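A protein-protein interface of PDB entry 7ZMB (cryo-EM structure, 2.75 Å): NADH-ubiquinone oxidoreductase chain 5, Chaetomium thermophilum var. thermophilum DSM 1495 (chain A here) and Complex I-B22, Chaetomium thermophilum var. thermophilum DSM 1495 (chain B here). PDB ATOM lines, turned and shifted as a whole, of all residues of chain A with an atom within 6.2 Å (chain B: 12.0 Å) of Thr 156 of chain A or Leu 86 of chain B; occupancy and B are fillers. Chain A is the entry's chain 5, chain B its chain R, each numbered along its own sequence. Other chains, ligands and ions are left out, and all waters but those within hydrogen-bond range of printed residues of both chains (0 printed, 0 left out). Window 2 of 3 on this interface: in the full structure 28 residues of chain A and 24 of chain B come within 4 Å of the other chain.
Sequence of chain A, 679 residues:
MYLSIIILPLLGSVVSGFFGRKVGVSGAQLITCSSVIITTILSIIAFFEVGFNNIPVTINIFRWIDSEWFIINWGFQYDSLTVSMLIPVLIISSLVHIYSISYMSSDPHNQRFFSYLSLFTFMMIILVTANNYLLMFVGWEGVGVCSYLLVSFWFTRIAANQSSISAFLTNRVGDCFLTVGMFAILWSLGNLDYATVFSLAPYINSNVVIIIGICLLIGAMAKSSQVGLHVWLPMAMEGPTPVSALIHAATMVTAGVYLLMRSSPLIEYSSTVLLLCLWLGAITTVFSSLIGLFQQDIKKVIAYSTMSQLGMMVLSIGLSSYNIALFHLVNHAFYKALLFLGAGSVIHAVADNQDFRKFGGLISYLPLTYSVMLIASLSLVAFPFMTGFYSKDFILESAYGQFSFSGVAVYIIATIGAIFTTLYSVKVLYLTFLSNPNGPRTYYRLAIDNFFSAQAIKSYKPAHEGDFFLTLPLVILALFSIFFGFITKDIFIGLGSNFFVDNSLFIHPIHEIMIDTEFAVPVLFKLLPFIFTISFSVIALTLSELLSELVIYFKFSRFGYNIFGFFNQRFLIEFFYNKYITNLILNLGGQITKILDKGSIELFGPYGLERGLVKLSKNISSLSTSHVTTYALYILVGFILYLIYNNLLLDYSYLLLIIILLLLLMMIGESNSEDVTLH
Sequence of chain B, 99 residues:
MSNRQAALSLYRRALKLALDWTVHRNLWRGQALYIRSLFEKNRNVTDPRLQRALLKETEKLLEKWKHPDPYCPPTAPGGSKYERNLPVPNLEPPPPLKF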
ATOM      1  N   PHE A 153       5.908  32.604 -24.456  1.00  0.00           N
ATOM      2  CA  PHE A 153       5.489  31.326 -25.014  1.00  0.00           C
ATOM      3  C   PHE A 153       5.545  30.234 -23.959  1.00  0.00           C
ATOM      4  O   PHE A 153       4.663  29.369 -23.900  1.00  0.00           O
ATOM      5  CB  PHE A 153       6.357  30.961 -26.212  1.00  0.00           C
ATOM      6  CG  PHE A 153       6.038  29.623 -26.794  1.00  0.00           C
ATOM      7  CD1 PHE A 153       4.830  29.403 -27.415  1.00  0.00           C
ATOM      8  CD2 PHE A 153       6.938  28.580 -26.700  1.00  0.00           C
ATOM      9  CE1 PHE A 153       4.525  28.169 -27.941  1.00  0.00           C
ATOM     10  CE2 PHE A 153       6.641  27.348 -27.228  1.00  0.00           C
ATOM     11  CZ  PHE A 153       5.433  27.142 -27.851  1.00  0.00           C
ATOM     12  N   TRP A 154       6.587  30.247 -23.131  1.00  0.00           N
ATOM     13  CA  TRP A 154       6.635  29.435 -21.921  1.00  0.00           C
ATOM     14  C   TRP A 154       6.036  30.253 -20.783  1.00  0.00           C
ATOM     15  O   TRP A 154       6.726  30.775 -19.913  1.00  0.00           O
ATOM     16  CB  TRP A 154       8.066  29.016 -21.606  1.00  0.00           C
ATOM     17  CG  TRP A 154       8.658  28.092 -22.590  1.00  0.00           C
ATOM     18  CD1 TRP A 154       8.237  26.842 -22.889  1.00  0.00           C
ATOM     19  CD2 TRP A 154       9.815  28.332 -23.396  1.00  0.00           C
ATOM     20  NE1 TRP A 154       9.047  26.282 -23.844  1.00  0.00           N
ATOM     21  CE2 TRP A 154      10.025  27.182 -24.172  1.00  0.00           C
ATOM     22  CE3 TRP A 154      10.685  29.411 -23.543  1.00  0.00           C
ATOM     23  CZ2 TRP A 154      11.067  27.081 -25.081  1.00  0.00           C
ATOM     24  CZ3 TRP A 154      11.717  29.305 -24.442  1.00  0.00           C
ATOM     25  CH2 TRP A 154      11.901  28.150 -25.199  1.00  0.00           C
ATOM     26  N   PHE A 155       4.712  30.366 -20.813  1.00  0.00           N
ATOM     27  CA  PHE A 155       4.046  31.277 -19.893  1.00  0.00           C
ATOM     28  C   PHE A 155       4.102  30.815 -18.443  1.00  0.00           C
ATOM     29  O   PHE A 155       3.649  31.554 -17.565  1.00  0.00           O
ATOM     30  CB  PHE A 155       2.599  31.502 -20.329  1.00  0.00           C
ATOM     31  CG  PHE A 155       1.817  30.247 -20.540  1.00  0.00           C
ATOM     32  CD1 PHE A 155       1.244  29.584 -19.475  1.00  0.00           C
ATOM     33  CD2 PHE A 155       1.634  29.737 -21.807  1.00  0.00           C
ATOM     34  CE1 PHE A 155       0.514  28.441 -19.671  1.00  0.00           C
ATOM     35  CE2 PHE A 155       0.906  28.592 -21.997  1.00  0.00           C
ATOM     36  CZ  PHE A 155       0.348  27.946 -20.927  1.00  0.00           C
ATOM     37  N   THR A 156       4.629  29.623 -18.165  1.00  0.00           N
ATOM     38  CA  THR A 156       4.879  29.249 -16.780  1.00  0.00           C
ATOM     39  C   THR A 156       6.202  29.799 -16.251  1.00  0.00           C
ATOM     40  O   THR A 156       6.415  29.806 -15.035  1.00  0.00           O
ATOM     41  CB  THR A 156       4.821  27.733 -16.628  1.00  0.00           C
ATOM     42  OG1 THR A 156       5.927  27.135 -17.312  1.00  0.00           O
ATOM     43  CG2 THR A 156       3.525  27.201 -17.211  1.00  0.00           C
ATOM     44  N   ARG A 157       7.077  30.268 -17.134  1.00  0.00           N
ATOM     45  CA  ARG A 157       8.154  31.188 -16.790  1.00  0.00           C
ATOM     46  C   ARG A 157       7.539  32.495 -16.309  1.00  0.00           C
ATOM     47  O   ARG A 157       6.937  33.223 -17.103  1.00  0.00           O
ATOM     48  CB  ARG A 157       9.012  31.478 -18.017  1.00  0.00           C
ATOM     49  CG  ARG A 157       9.767  30.334 -18.623  1.00  0.00           C
ATOM     50  CD  ARG A 157      10.911  29.920 -17.781  1.00  0.00           C
ATOM     51  NE  ARG A 157      11.901  30.992 -17.738  1.00  0.00           N
ATOM     52  CZ  ARG A 157      12.878  31.078 -16.844  1.00  0.00           C
ATOM     53  NH1 ARG A 157      13.009  30.149 -15.911  1.00  0.00           N
ATOM     54  NH2 ARG A 157      13.730  32.093 -16.890  1.00  0.00           N
ATOM     55  N   ILE A 158       7.695  32.805 -15.024  1.00  0.00           N
ATOM     56  CA  ILE A 158       7.379  34.157 -14.579  1.00  0.00           C
ATOM     57  C   ILE A 158       8.271  35.167 -15.290  1.00  0.00           C
ATOM     58  O   ILE A 158       7.837  36.276 -15.625  1.00  0.00           O
ATOM     59  CB  ILE A 158       7.498  34.262 -13.049  1.00  0.00           C
ATOM     60  CG1 ILE A 158       6.347  33.513 -12.379  1.00  0.00           C
ATOM     61  CG2 ILE A 158       7.558  35.708 -12.604  1.00  0.00           C
ATOM     62  CD1 ILE A 158       6.499  33.383 -10.897  1.00  0.00           C
ATOM     63  N   ALA A 159       9.525  34.793 -15.548  1.00  0.00           N
ATOM     64  CA  ALA A 159      10.448  35.687 -16.232  1.00  0.00           C
ATOM     65  C   ALA A 159       9.949  36.037 -17.624  1.00  0.00           C
ATOM     66  O   ALA A 159      10.032  37.195 -18.047  1.00  0.00           O
ATOM     67  CB  ALA A 159      11.834  35.049 -16.303  1.00  0.00           C
ATOM     68  N   ASN A 161       6.890  36.141 -18.415  1.00  0.00           N
ATOM     69  CA  ASN A 161       5.715  36.980 -18.217  1.00  0.00           C
ATOM     70  C   ASN A 161       6.098  38.439 -18.029  1.00  0.00           C
ATOM     71  O   ASN A 161       5.542  39.323 -18.691  1.00  0.00           O
ATOM     72  CB  ASN A 161       4.910  36.477 -17.024  1.00  0.00           C
ATOM     73  CG  ASN A 161       4.072  35.289 -17.369  1.00  0.00           C
ATOM     74  OD1 ASN A 161       2.883  35.413 -17.632  1.00  0.00           O
ATOM     75  ND2 ASN A 161       4.689  34.123 -17.395  1.00  0.00           N
ATOM     76  N   PRO B  74      20.560  26.182 -15.546  1.00  0.00           N
ATOM     77  CA  PRO B  74      19.269  26.596 -16.124  1.00  0.00           C
ATOM     78  C   PRO B  74      18.056  26.056 -15.388  1.00  0.00           C
ATOM     79  O   PRO B  74      17.046  26.757 -15.287  1.00  0.00           O
ATOM     80  CB  PRO B  74      19.346  26.063 -17.560  1.00  0.00           C
ATOM     81  CG  PRO B  74      20.811  25.880 -17.827  1.00  0.00           C
ATOM     82  CD  PRO B  74      21.408  25.479 -16.521  1.00  0.00           C
ATOM     83  N   THR B  75      18.118  24.831 -14.877  1.00  0.00           N
ATOM     84  CA  THR B  75      16.977  24.219 -14.196  1.00  0.00           C
ATOM     85  C   THR B  75      17.042  24.505 -12.695  1.00  0.00           C
ATOM     86  O   THR B  75      17.047  23.607 -11.854  1.00  0.00           O
ATOM     87  CB  THR B  75      16.941  22.720 -14.466  1.00  0.00           C
ATOM     88  OG1 THR B  75      18.126  22.113 -13.937  1.00  0.00           O
ATOM     89  CG2 THR B  75      16.875  22.453 -15.955  1.00  0.00           C
ATOM     90  N   ALA B  76      17.100  25.791 -12.371  1.00  0.00           N
ATOM     91  CA  ALA B  76      17.326  26.225 -11.005  1.00  0.00           C
ATOM     92  C   ALA B  76      16.724  27.606 -10.833  1.00  0.00           C
ATOM     93  O   ALA B  76      16.613  28.354 -11.810  1.00  0.00           O
ATOM     94  CB  ALA B  76      18.822  26.257 -10.667  1.00  0.00           C
ATOM     95  N   PRO B  77      16.320  27.970  -9.619  1.00  0.00           N
ATOM     96  CA  PRO B  77      15.795  29.323  -9.393  1.00  0.00           C
ATOM     97  C   PRO B  77      16.800  30.374  -9.837  1.00  0.00           C
ATOM     98  O   PRO B  77      17.911  30.462  -9.310  1.00  0.00           O
ATOM     99  CB  PRO B  77      15.561  29.357  -7.882  1.00  0.00           C
ATOM    100  CG  PRO B  77      15.329  27.925  -7.517  1.00  0.00           C
ATOM    101  CD  PRO B  77      16.227  27.129  -8.415  1.00  0.00           C
ATOM    102  N   GLY B  78      16.395  31.178 -10.816  1.00  0.00           N
ATOM    103  CA  GLY B  78      17.301  32.075 -11.492  1.00  0.00           C
ATOM    104  C   GLY B  78      17.936  31.495 -12.735  1.00  0.00           C
ATOM    105  O   GLY B  78      18.577  32.237 -13.490  1.00  0.00           O
ATOM    106  N   GLY B  79      17.779  30.190 -12.971  1.00  0.00           N
ATOM    107  CA  GLY B  79      18.259  29.588 -14.193  1.00  0.00           C
ATOM    108  C   GLY B  79      17.370  29.909 -15.369  1.00  0.00           C
ATOM    109  O   GLY B  79      16.278  30.456 -15.229  1.00  0.00           O
ATOM    110  N   SER B  80      17.857  29.560 -16.557  1.00  0.00           N
ATOM    111  CA  SER B  80      17.130  29.881 -17.777  1.00  0.00           C
ATOM    112  C   SER B  80      15.922  28.973 -17.966  1.00  0.00           C
ATOM    113  O   SER B  80      14.854  29.437 -18.376  1.00  0.00           O
ATOM    114  CB  SER B  80      18.065  29.787 -18.981  1.00  0.00           C
ATOM    115  OG  SER B  80      17.351  29.913 -20.198  1.00  0.00           O
ATOM    116  N   LYS B  81      16.066  27.685 -17.678  1.00  0.00           N
ATOM    117  CA  LYS B  81      15.026  26.705 -17.955  1.00  0.00           C
ATOM    118  C   LYS B  81      14.102  26.483 -16.759  1.00  0.00           C
ATOM    119  O   LYS B  81      13.176  25.674 -16.845  1.00  0.00           O
ATOM    120  CB  LYS B  81      15.673  25.388 -18.407  1.00  0.00           C
ATOM    121  CG  LYS B  81      14.713  24.293 -18.869  1.00  0.00           C
ATOM    122  CD  LYS B  81      15.444  23.018 -19.228  1.00  0.00           C
ATOM    123  CE  LYS B  81      16.176  23.166 -20.541  1.00  0.00           C
ATOM    124  NZ  LYS B  81      16.805  21.889 -20.971  1.00  0.00           N
ATOM    125  N   TYR B  82      14.319  27.199 -15.660  1.00  0.00           N
ATOM    126  CA  TYR B  82      13.484  27.042 -14.476  1.00  0.00           C
ATOM    127  C   TYR B  82      12.017  27.297 -14.794  1.00  0.00           C
ATOM    128  O   TYR B  82      11.679  28.247 -15.499  1.00  0.00           O
ATOM    129  CB  TYR B  82      13.936  28.002 -13.383  1.00  0.00           C
ATOM    130  CG  TYR B  82      13.139  27.882 -12.110  1.00  0.00           C
ATOM    131  CD1 TYR B  82      13.049  26.675 -11.436  1.00  0.00           C
ATOM    132  CD2 TYR B  82      12.460  28.973 -11.592  1.00  0.00           C
ATOM    133  CE1 TYR B  82      12.316  26.559 -10.275  1.00  0.00           C
ATOM    134  CE2 TYR B  82      11.719  28.868 -10.430  1.00  0.00           C
ATOM    135  CZ  TYR B  82      11.652  27.658  -9.775  1.00  0.00           C
ATOM    136  OH  TYR B  82      10.921  27.543  -8.617  1.00  0.00           O
ATOM    137  N   GLU B  83      11.148  26.439 -14.256  1.00  0.00           N
ATOM    138  CA  GLU B  83       9.695  26.475 -14.436  1.00  0.00           C
ATOM    139  C   GLU B  83       9.282  26.748 -15.880  1.00  0.00           C
ATOM    140  O   GLU B  83       8.334  27.493 -16.123  1.00  0.00           O
ATOM    141  CB  GLU B  83       9.044  27.491 -13.475  1.00  0.00           C
ATOM    142  CG  GLU B  83       9.449  28.952 -13.630  1.00  0.00           C
ATOM    143  CD  GLU B  83       8.722  29.873 -12.672  1.00  0.00           C
ATOM    144  OE1 GLU B  83       7.997  29.366 -11.792  1.00  0.00           O
ATOM    145  OE2 GLU B  83       8.868  31.104 -12.803  1.00  0.00           O
ATOM    146  N   ARG B  84       9.956  26.104 -16.838  1.00  0.00           N
ATOM    147  CA  ARG B  84       9.710  26.360 -18.255  1.00  0.00           C
ATOM    148  C   ARG B  84       8.490  25.609 -18.776  1.00  0.00           C
ATOM    149  O   ARG B  84       7.539  26.218 -19.277  1.00  0.00           O
ATOM    150  CB  ARG B  84      10.936  25.979 -19.081  1.00  0.00           C
ATOM    151  CG  ARG B  84      10.641  25.842 -20.565  1.00  0.00           C
ATOM    152  CD  ARG B  84      11.891  25.602 -21.363  1.00  0.00           C
ATOM    153  NE  ARG B  84      12.653  26.829 -21.545  1.00  0.00           N
ATOM    154  CZ  ARG B  84      13.850  26.883 -22.113  1.00  0.00           C
ATOM    155  NH1 ARG B  84      14.426  25.776 -22.552  1.00  0.00           N
ATOM    156  NH2 ARG B  84      14.472  28.043 -22.238  1.00  0.00           N
ATOM    157  N   ASN B  85       8.515  24.282 -18.693  1.00  0.00           N
ATOM    158  CA  ASN B  85       7.444  23.426 -19.197  1.00  0.00           C
ATOM    159  C   ASN B  85       6.828  22.734 -17.988  1.00  0.00           C
ATOM    160  O   ASN B  85       7.207  21.615 -17.637  1.00  0.00           O
ATOM    161  CB  ASN B  85       7.973  22.425 -20.211  1.00  0.00           C
ATOM    162  CG  ASN B  85       8.581  23.092 -21.425  1.00  0.00           C
ATOM    163  OD1 ASN B  85       8.087  24.115 -21.894  1.00  0.00           O
ATOM    164  ND2 ASN B  85       9.662  22.520 -21.936  1.00  0.00           N
ATOM    165  N   LEU B  86       5.895  23.393 -17.365  1.00  0.00           N
ATOM    166  CA  LEU B  86       5.376  22.886 -16.108  1.00  0.00           C
ATOM    167  C   LEU B  86       4.146  22.025 -16.348  1.00  0.00           C
ATOM    168  O   LEU B  86       3.199  22.480 -16.999  1.00  0.00           O
ATOM    169  CB  LEU B  86       5.029  24.032 -15.173  1.00  0.00           C
ATOM    170  CG  LEU B  86       6.226  24.821 -14.659  1.00  0.00           C
ATOM    171  CD1 LEU B  86       5.780  25.906 -13.691  1.00  0.00           C
ATOM    172  CD2 LEU B  86       7.221  23.884 -13.999  1.00  0.00           C
ATOM    173  N   PRO B  87       4.125  20.793 -15.853  1.00  0.00           N
ATOM    174  CA  PRO B  87       2.902  19.992 -15.928  1.00  0.00           C
ATOM    175  C   PRO B  87       1.829  20.574 -15.024  1.00  0.00           C
ATOM    176  O   PRO B  87       2.109  21.293 -14.066  1.00  0.00           O
ATOM    177  CB  PRO B  87       3.349  18.611 -15.442  1.00  0.00           C
ATOM    178  CG  PRO B  87       4.504  18.893 -14.554  1.00  0.00           C
ATOM    179  CD  PRO B  87       5.200  20.095 -15.128  1.00  0.00           C
ATOM    180  N   VAL B  88       0.585  20.262 -15.349  1.00  0.00           N
ATOM    181  CA  VAL B  88      -0.507  20.766 -14.513  1.00  0.00           C
ATOM    182  C   VAL B  88      -0.438  20.092 -13.148  1.00  0.00           C
ATOM    183  O   VAL B  88      -0.155  18.883 -13.066  1.00  0.00           O
ATOM    184  CB  VAL B  88      -1.859  20.530 -15.189  1.00  0.00           C
ATOM    185  CG1 VAL B  88      -1.811  21.005 -16.631  1.00  0.00           C
ATOM    186  CG2 VAL B  88      -2.289  19.085 -15.083  1.00  0.00           C
ATOM    187  N   PRO B  89      -0.610  20.829 -12.056  1.00  0.00           N
ATOM    188  CA  PRO B  89      -0.514  20.202 -10.730  1.00  0.00           C
ATOM    189  C   PRO B  89      -1.566  19.137 -10.477  1.00  0.00           C
ATOM    190  O   PRO B  89      -1.359  18.270  -9.618  1.00  0.00           O
ATOM    191  CB  PRO B  89      -0.673  21.391  -9.774  1.00  0.00           C
ATOM    192  CG  PRO B  89      -0.221  22.570 -10.575  1.00  0.00           C
ATOM    193  CD  PRO B  89      -0.644  22.296 -11.982  1.00  0.00           C
ATOM    194  N   ASN B  90      -2.685  19.172 -11.194  1.00  0.00           N
ATOM    195  CA  ASN B  90      -3.824  18.299 -10.940  1.00  0.00           C
ATOM    196  C   ASN B  90      -4.144  17.543 -12.221  1.00  0.00           C
ATOM    197  O   ASN B  90      -4.713  18.113 -13.158  1.00  0.00           O
ATOM    198  CB  ASN B  90      -5.018  19.121 -10.456  1.00  0.00           C
ATOM    199  CG  ASN B  90      -6.214  18.277 -10.116  1.00  0.00           C
ATOM    200  OD1 ASN B  90      -6.132  17.060 -10.062  1.00  0.00           O
ATOM    201  ND2 ASN B  90      -7.338  18.927  -9.867  1.00  0.00           N
ATOM    202  N   LEU B  91      -3.789  16.260 -12.260  1.00  0.00           N
ATOM    203  CA  LEU B  91      -4.002  15.450 -13.451  1.00  0.00           C
ATOM    204  C   LEU B  91      -5.381  14.817 -13.520  1.00  0.00           C
ATOM    205  O   LEU B  91      -5.763  14.335 -14.590  1.00  0.00           O
ATOM    206  CB  LEU B  91      -2.950  14.340 -13.541  1.00  0.00           C
ATOM    207  CG  LEU B  91      -1.580  14.664 -14.138  1.00  0.00           C
ATOM    208  CD1 LEU B  91      -1.732  15.053 -15.601  1.00  0.00           C
ATOM    209  CD2 LEU B  91      -0.864  15.757 -13.362  1.00  0.00           C
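O of Pro 74 of chain B sits at hydrogen-bond distance from N of Tyr 82 of chain B, at 2.8 Å.
O of Pro 74 of chain B lies within hydrogen-bond range of N of Lys 81 of chain B, 2.7 Å away.
The backbone carbonyl oxygen (O) of Arg 157 of chain A is in hydrogen-bond range of the side-chain amide nitrogen (ND2) of Asn 161 of chain A (2.4 Å).
The backbone NH of Ser 80 of chain B sits at hydrogen-bond distance from the backbone carbonyl oxygen of Pro 74 of chain B, at 3.2 Å.
Of chain B, only Glu 83, Arg 84 and Leu 86 come within 4 Å of Thr 156 of chain A.
Of chain A, only Thr 156 comes within 4 Å of Leu 86 of chain B.
Phe 155 of chain A touches none of the printed residues of chain B.
Of chain B, only Gly 79 (3.4 Å), Ser 80 (3.0 Å), Lys 81 (3.9 Å), Tyr 82 (2.4 Å), Glu 83 (3.2 Å) and Arg 84 (3.8 Å) come within 4 Å of Arg 157 of chain A.
Of the printed residues of chain A, Gly 79 of chain B touches Arg 157 (3.4 Å).
Of the printed residues of chain A, Asn 85 of chain B touches Trp 154.
Of the printed residues of chain A, Tyr 82 of chain B touches Arg 157 (2.4 Å).
Asn 90 of chain B touches none of the printed residues of chain A.
Pro 87 of chain B touches none of the printed residues of chain A.
The nearest residue of chain A that does not touch Leu 86 of chain B is Arg 157 of chain A (5.7 Å).
Along chain A the printed residues that touch a printed residue of chain B span positions 154 to 158.
Hydrophobic or aromatic side chains of chain B that line the printed part of chain A: Tyr 82 and Leu 86.
Among the printed residues, 12 pairs touch across the chains.
CD1 of Trp 154 of chain A touches CG of Arg 84 of chain B, 3.5 Å away.
Thr 156 of chain A touches Leu 86 of chain B.
NH1 of Arg 157 of chain A touches C of Lys 81 of chain B, 3.9 Å away.
CA of Arg 84 of chain B touches CD of Arg 157 of chain A (3.8 Å).
The indole nitrogen (NE1) of Trp 154 of chain A lies close to the side-chain amide oxygen (OD1) of Asn 85 of chain B (3.1 Å).
The backbone carbonyl oxygen of Glu 83 of chain B lies within hydrogen-bond range of the side-chain hydroxyl of Thr 156 of chain A (2.7 Å).
The side-chain carboxylate (OE2) of Glu 83 of chain B sits at hydrogen-bond distance from the backbone NH (N) of Ile 158 of chain A (3.0 Å).
The guanidinium group (NH1) of Arg 157 of chain A is in hydrogen-bond range of the backbone carbonyl oxygen (O) of Gly 79 of chain B, 3.4 Å away.
The side-chain hydroxyl (OG1) of Thr 156 of chain A lies within hydrogen-bond range of the backbone carbonyl oxygen (O) of Arg 84 of chain B (2.7 Å).
The backbone carbonyl oxygen of Ser 80 of chain B lies close to the guanidinium group of Arg 157 of chain A (3.2 Å).
The backbone carbonyl oxygen (O) of Glu 83 of chain B sits at hydrogen-bond distance from the backbone NH (N) of Arg 157 of chain A.
NH1 of Arg 157 of chain A sits close to O of Tyr 82 of chain B (2.4 Å).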
